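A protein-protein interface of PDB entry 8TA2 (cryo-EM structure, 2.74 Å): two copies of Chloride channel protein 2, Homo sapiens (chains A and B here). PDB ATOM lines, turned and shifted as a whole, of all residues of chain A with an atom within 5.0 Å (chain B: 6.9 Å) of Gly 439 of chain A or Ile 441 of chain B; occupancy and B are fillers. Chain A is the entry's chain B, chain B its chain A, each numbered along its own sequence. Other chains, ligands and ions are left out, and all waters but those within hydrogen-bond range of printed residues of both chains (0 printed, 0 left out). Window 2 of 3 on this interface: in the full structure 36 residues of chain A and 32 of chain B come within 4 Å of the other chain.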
ATOM      1  N   LYS A 220     -13.918  -7.599 -10.303  1.00  0.00           N
ATOM      2  CA  LYS A 220     -14.272  -6.243  -9.875  1.00  0.00           C
ATOM      3  C   LYS A 220     -15.585  -5.804 -10.511  1.00  0.00           C
ATOM      4  O   LYS A 220     -15.685  -5.663 -11.726  1.00  0.00           O
ATOM      5  CB  LYS A 220     -13.112  -5.286 -10.181  1.00  0.00           C
ATOM      6  CG  LYS A 220     -13.342  -3.879  -9.604  1.00  0.00           C
ATOM      7  CD  LYS A 220     -12.150  -2.931  -9.812  1.00  0.00           C
ATOM      8  CE  LYS A 220     -10.908  -3.369  -9.029  1.00  0.00           C
ATOM      9  NZ  LYS A 220      -9.786  -2.421  -9.178  1.00  0.00           N
ATOM     10  N   THR A 221     -16.594  -5.580  -9.685  1.00  0.00           N
ATOM     11  CA  THR A 221     -17.917  -5.083 -10.091  1.00  0.00           C
ATOM     12  C   THR A 221     -17.912  -3.575 -10.359  1.00  0.00           C
ATOM     13  O   THR A 221     -17.093  -2.843  -9.813  1.00  0.00           O
ATOM     14  CB  THR A 221     -18.971  -5.433  -9.043  1.00  0.00           C
ATOM     15  OG1 THR A 221     -18.620  -4.897  -7.796  1.00  0.00           O
ATOM     16  CG2 THR A 221     -19.166  -6.938  -8.903  1.00  0.00           C
ATOM     17  N   VAL A 434     -16.518 -11.295  -0.250  1.00  0.00           N
ATOM     18  CA  VAL A 434     -17.163 -10.674  -1.415  1.00  0.00           C
ATOM     19  C   VAL A 434     -16.856  -9.187  -1.559  1.00  0.00           C
ATOM     20  O   VAL A 434     -16.775  -8.724  -2.690  1.00  0.00           O
ATOM     21  CB  VAL A 434     -18.667 -10.939  -1.534  1.00  0.00           C
ATOM     22  CG1 VAL A 434     -18.923 -12.428  -1.725  1.00  0.00           C
ATOM     23  CG2 VAL A 434     -19.513 -10.405  -0.391  1.00  0.00           C
ATOM     24  N   PHE A 435     -16.607  -8.432  -0.487  1.00  0.00           N
ATOM     25  CA  PHE A 435     -16.155  -7.046  -0.607  1.00  0.00           C
ATOM     26  C   PHE A 435     -14.742  -6.947  -1.180  1.00  0.00           C
ATOM     27  O   PHE A 435     -14.519  -6.212  -2.136  1.00  0.00           O
ATOM     28  CB  PHE A 435     -16.245  -6.339   0.745  1.00  0.00           C
ATOM     29  CG  PHE A 435     -17.597  -6.413   1.427  1.00  0.00           C
ATOM     30  CD1 PHE A 435     -18.787  -6.393   0.673  1.00  0.00           C
ATOM     31  CD2 PHE A 435     -17.667  -6.525   2.826  1.00  0.00           C
ATOM     32  CE1 PHE A 435     -20.029  -6.564   1.302  1.00  0.00           C
ATOM     33  CE2 PHE A 435     -18.913  -6.689   3.453  1.00  0.00           C
ATOM     34  CZ  PHE A 435     -20.088  -6.743   2.690  1.00  0.00           C
ATOM     35  N   GLU A 436     -13.781  -7.702  -0.656  1.00  0.00           N
ATOM     36  CA  GLU A 436     -12.412  -7.705  -1.181  1.00  0.00           C
ATOM     37  C   GLU A 436     -12.339  -8.203  -2.621  1.00  0.00           C
ATOM     38  O   GLU A 436     -11.541  -7.708  -3.405  1.00  0.00           O
ATOM     39  CB  GLU A 436     -11.528  -8.622  -0.337  1.00  0.00           C
ATOM     40  CG  GLU A 436     -11.267  -8.060   1.053  1.00  0.00           C
ATOM     41  CD  GLU A 436     -10.498  -9.077   1.902  1.00  0.00           C
ATOM     42  OE1 GLU A 436     -11.087 -10.101   2.296  1.00  0.00           O
ATOM     43  OE2 GLU A 436      -9.298  -8.864   2.167  1.00  0.00           O
ATOM     44  N   LEU A 437     -13.176  -9.177  -2.977  1.00  0.00           N
ATOM     45  CA  LEU A 437     -13.264  -9.792  -4.296  1.00  0.00           C
ATOM     46  C   LEU A 437     -13.974  -8.881  -5.312  1.00  0.00           C
ATOM     47  O   LEU A 437     -13.390  -8.459  -6.296  1.00  0.00           O
ATOM     48  CB  LEU A 437     -13.991 -11.129  -4.100  1.00  0.00           C
ATOM     49  CG  LEU A 437     -14.165 -11.992  -5.351  1.00  0.00           C
ATOM     50  CD1 LEU A 437     -12.859 -12.649  -5.749  1.00  0.00           C
ATOM     51  CD2 LEU A 437     -15.190 -13.066  -5.047  1.00  0.00           C
ATOM     52  N   THR A 438     -15.229  -8.497  -5.069  1.00  0.00           N
ATOM     53  CA  THR A 438     -15.973  -7.627  -5.991  1.00  0.00           C
ATOM     54  C   THR A 438     -15.456  -6.198  -6.048  1.00  0.00           C
ATOM     55  O   THR A 438     -15.868  -5.449  -6.931  1.00  0.00           O
ATOM     56  CB  THR A 438     -17.458  -7.569  -5.669  1.00  0.00           C
ATOM     57  OG1 THR A 438     -17.672  -6.965  -4.427  1.00  0.00           O
ATOM     58  CG2 THR A 438     -18.114  -8.943  -5.709  1.00  0.00           C
ATOM     59  N   GLY A 439     -14.559  -5.812  -5.134  1.00  0.00           N
ATOM     60  CA  GLY A 439     -13.865  -4.528  -5.114  1.00  0.00           C
ATOM     61  C   GLY A 439     -14.720  -3.351  -4.649  1.00  0.00           C
ATOM     62  O   GLY A 439     -14.305  -2.210  -4.820  1.00  0.00           O
ATOM     63  N   GLN A 440     -15.905  -3.602  -4.091  1.00  0.00           N
ATOM     64  CA  GLN A 440     -16.889  -2.592  -3.715  1.00  0.00           C
ATOM     65  C   GLN A 440     -17.576  -2.949  -2.397  1.00  0.00           C
ATOM     66  O   GLN A 440     -17.659  -4.117  -2.032  1.00  0.00           O
ATOM     67  CB  GLN A 440     -17.937  -2.424  -4.827  1.00  0.00           C
ATOM     68  CG  GLN A 440     -17.375  -1.880  -6.150  1.00  0.00           C
ATOM     69  CD  GLN A 440     -18.445  -1.213  -7.011  1.00  0.00           C
ATOM     70  OE1 GLN A 440     -19.616  -1.553  -6.997  1.00  0.00           O
ATOM     71  NE2 GLN A 440     -18.097  -0.192  -7.759  1.00  0.00           N
ATOM     72  N   ILE A 441     -18.088  -1.935  -1.693  1.00  0.00           N
ATOM     73  CA  ILE A 441     -18.727  -2.047  -0.366  1.00  0.00           C
ATOM     74  C   ILE A 441     -20.191  -1.557  -0.365  1.00  0.00           C
ATOM     75  O   ILE A 441     -20.917  -1.779   0.596  1.00  0.00           O
ATOM     76  CB  ILE A 441     -17.798  -1.374   0.686  1.00  0.00           C
ATOM     77  CG1 ILE A 441     -16.681  -2.380   1.034  1.00  0.00           C
ATOM     78  CG2 ILE A 441     -18.482  -0.884   1.972  1.00  0.00           C
ATOM     79  CD1 ILE A 441     -15.559  -1.840   1.908  1.00  0.00           C
ATOM     80  N   LEU B 225     -11.247   4.760  -9.228  1.00  0.00           N
ATOM     81  CA  LEU B 225     -11.254   3.292  -9.240  1.00  0.00           C
ATOM     82  C   LEU B 225     -10.134   2.708 -10.119  1.00  0.00           C
ATOM     83  O   LEU B 225      -9.724   1.569  -9.907  1.00  0.00           O
ATOM     84  CB  LEU B 225     -12.637   2.785  -9.675  1.00  0.00           C
ATOM     85  CG  LEU B 225     -13.778   3.136  -8.703  1.00  0.00           C
ATOM     86  CD1 LEU B 225     -15.116   2.704  -9.297  1.00  0.00           C
ATOM     87  CD2 LEU B 225     -13.617   2.453  -7.349  1.00  0.00           C
ATOM     88  N   PHE B 435     -12.133   0.903   5.572  1.00  0.00           N
ATOM     89  CA  PHE B 435     -12.875   0.621   4.345  1.00  0.00           C
ATOM     90  C   PHE B 435     -14.377   0.847   4.503  1.00  0.00           C
ATOM     91  O   PHE B 435     -15.003   1.421   3.620  1.00  0.00           O
ATOM     92  CB  PHE B 435     -12.623  -0.813   3.877  1.00  0.00           C
ATOM     93  CG  PHE B 435     -11.176  -1.227   3.741  1.00  0.00           C
ATOM     94  CD1 PHE B 435     -10.213  -0.343   3.214  1.00  0.00           C
ATOM     95  CD2 PHE B 435     -10.792  -2.519   4.142  1.00  0.00           C
ATOM     96  CE1 PHE B 435      -8.865  -0.730   3.155  1.00  0.00           C
ATOM     97  CE2 PHE B 435      -9.445  -2.904   4.083  1.00  0.00           C
ATOM     98  CZ  PHE B 435      -8.480  -1.995   3.626  1.00  0.00           C
ATOM     99  N   THR B 438     -14.810   4.815   4.791  1.00  0.00           N
ATOM    100  CA  THR B 438     -14.549   5.524   3.540  1.00  0.00           C
ATOM    101  C   THR B 438     -15.396   5.025   2.375  1.00  0.00           C
ATOM    102  O   THR B 438     -15.447   5.706   1.354  1.00  0.00           O
ATOM    103  CB  THR B 438     -13.072   5.487   3.152  1.00  0.00           C
ATOM    104  OG1 THR B 438     -12.629   4.178   2.968  1.00  0.00           O
ATOM    105  CG2 THR B 438     -12.189   6.175   4.181  1.00  0.00           C
ATOM    106  N   GLY B 439     -16.079   3.882   2.508  1.00  0.00           N
ATOM    107  CA  GLY B 439     -16.953   3.290   1.493  1.00  0.00           C
ATOM    108  C   GLY B 439     -16.228   2.683   0.291  1.00  0.00           C
ATOM    109  O   GLY B 439     -16.865   2.386  -0.715  1.00  0.00           O
ATOM    110  N   GLN B 440     -14.910   2.523   0.367  1.00  0.00           N
ATOM    111  CA  GLN B 440     -14.035   2.099  -0.719  1.00  0.00           C
ATOM    112  C   GLN B 440     -12.956   1.153  -0.190  1.00  0.00           C
ATOM    113  O   GLN B 440     -12.522   1.273   0.952  1.00  0.00           O
ATOM    114  CB  GLN B 440     -13.373   3.317  -1.376  1.00  0.00           C
ATOM    115  CG  GLN B 440     -14.347   4.258  -2.104  1.00  0.00           C
ATOM    116  CD  GLN B 440     -13.654   5.122  -3.156  1.00  0.00           C
ATOM    117  OE1 GLN B 440     -12.466   5.395  -3.112  1.00  0.00           O
ATOM    118  NE2 GLN B 440     -14.354   5.552  -4.179  1.00  0.00           N
ATOM    119  N   ILE B 441     -12.502   0.220  -1.030  1.00  0.00           N
ATOM    120  CA  ILE B 441     -11.546  -0.841  -0.672  1.00  0.00           C
ATOM    121  C   ILE B 441     -10.348  -0.906  -1.641  1.00  0.00           C
ATOM    122  O   ILE B 441      -9.575  -1.853  -1.635  1.00  0.00           O
ATOM    123  CB  ILE B 441     -12.319  -2.161  -0.419  1.00  0.00           C
ATOM    124  CG1 ILE B 441     -11.474  -3.249   0.274  1.00  0.00           C
ATOM    125  CG2 ILE B 441     -12.943  -2.720  -1.700  1.00  0.00           C
ATOM    126  CD1 ILE B 441     -12.316  -4.277   1.037  1.00  0.00           C
ATOM    127  N   ALA B 442     -10.133   0.128  -2.457  1.00  0.00           N
ATOM    128  CA  ALA B 442      -9.037   0.191  -3.429  1.00  0.00           C
ATOM    129  C   ALA B 442      -7.629   0.353  -2.816  1.00  0.00           C
ATOM    130  O   ALA B 442      -6.652  -0.108  -3.394  1.00  0.00           O
ATOM    131  CB  ALA B 442      -9.341   1.335  -4.399  1.00  0.00           C
ATOM    132  N   HIS B 443      -7.498   0.981  -1.644  1.00  0.00           N
ATOM    133  CA  HIS B 443      -6.222   1.210  -0.936  1.00  0.00           C
ATOM    134  C   HIS B 443      -5.825   0.055   0.002  1.00  0.00           C
ATOM    135  O   HIS B 443      -4.948   0.216   0.843  1.00  0.00           O
ATOM    136  CB  HIS B 443      -6.263   2.576  -0.222  1.00  0.00           C
ATOM    137  CG  HIS B 443      -6.052   3.747  -1.144  1.00  0.00           C
ATOM    138  ND1 HIS B 443      -4.809   4.253  -1.524  1.00  0.00           N
ATOM    139  CD2 HIS B 443      -7.023   4.454  -1.781  1.00  0.00           C
ATOM    140  CE1 HIS B 443      -5.054   5.253  -2.379  1.00  0.00           C
ATOM    141  NE2 HIS B 443      -6.376   5.392  -2.551  1.00  0.00           N
ATOM    142  N   ILE B 444      -6.448  -1.120  -0.118  1.00  0.00           N
ATOM    143  CA  ILE B 444      -6.283  -2.245   0.810  1.00  0.00           C
ATOM    144  C   ILE B 444      -4.836  -2.704   1.021  1.00  0.00           C
ATOM    145  O   ILE B 444      -4.425  -2.852   2.166  1.00  0.00           O
ATOM    146  CB  ILE B 444      -7.243  -3.398   0.440  1.00  0.00           C
ATOM    147  CG1 ILE B 444      -7.107  -4.564   1.437  1.00  0.00           C
ATOM    148  CG2 ILE B 444      -7.050  -3.915  -0.998  1.00  0.00           C
ATOM    149  CD1 ILE B 444      -8.295  -5.523   1.423  1.00  0.00           C
ATOM    150  N   LEU B 445      -4.027  -2.870  -0.026  1.00  0.00           N
ATOM    151  CA  LEU B 445      -2.622  -3.253   0.133  1.00  0.00           C
ATOM    152  C   LEU B 445      -1.802  -2.178   0.877  1.00  0.00           C
ATOM    153  O   LEU B 445      -1.191  -2.532   1.884  1.00  0.00           O
ATOM    154  CB  LEU B 445      -2.023  -3.711  -1.212  1.00  0.00           C
ATOM    155  CG  LEU B 445      -0.531  -4.083  -1.140  1.00  0.00           C
ATOM    156  CD1 LEU B 445      -0.338  -5.401  -0.400  1.00  0.00           C
ATOM    157  CD2 LEU B 445       0.053  -4.224  -2.535  1.00  0.00           C
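The backbone carbonyl oxygen (O) of Phe 435 of chain B lies within hydrogen-bond range of the backbone NH (N) of Gln 440 of chain B (3.4 Å).
Phe 435 of chain A touches Ile 441 of chain B, and with the chains exchanged Ile 441 of chain A touches Phe 435 of chain B. Gly 439 of chain A touches Ile 441 of chain B, but with the chains exchanged Ile 441 of chain A does not touch Gly 439 of chain B (4.1 Å). Gln 440 of chain A touches Ile 441 of chain B, but with the chains exchanged Ile 441 of chain A does not touch Gln 440 of chain B (4.5 Å). 5 positions are printed for both chains.
Among the printed residues, merely in contact across the chains: Gly 439 of chain A with Ile 441 of chain B (3.4 Å), Glu 436 of chain A with Ile 444 of chain B (3.6 Å), Ile 441 of chain A with Phe 435 of chain B (3.7 Å), Phe 435 of chain A with Ile 441 of chain B (3.9 Å), Gln 440 of chain A with Ile 441 of chain B (3.9 Å) and Glu 436 of chain A with Ile 441 of chain B (3.9 Å).
Of the 10 printed residues of chain B, 3 touch a printed residue of chain A. Hydrophobic or aromatic side chains of chain B that line the printed part of chain A: Phe 435, Ile 441 and Ile 444. Of the 10 printed residues of chain A, 5 touch a printed residue of chain B. Printed residues of chain A that touch a printed residue of chain B: Phe 435, Glu 436, Gly 439, Gln 440 and Ile 441. Hydrophobic or aromatic side chains of chain A within 4 Å of the printed part of chain B: Ile 441. Among the printed residues, 6 pairs touch across the chains. Among the printed residues, no Asp or Glu carboxylate lies within 4 Å of a Lys or Arg side-chain nitrogen of the other chain.
Of the printed residues of chain B, Phe 435 of chain A touches Ile 441. Leu 437 of chain A touches none of the printed residues of chain B. Of chain B, only Ile 441 comes within 4 Å of Gly 439 of chain A. Printed residues of chain A within 4 Å of Ile 441 of chain B: Phe 435, Glu 436, Gly 439 and Gln 440. Ala 442 of chain B touches none of the printed residues of chain A. Of the printed residues of chain A, Ile 444 of chain B touches Glu 436 (3.6 Å). The nearest printed residue of chain A that does not touch Ile 441 of chain B is Ile 441 of chain A (4.002 Å). The nearest printed residue of chain A that does not touch Ile 444 of chain B is Phe 435 of chain A (7.1 Å).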
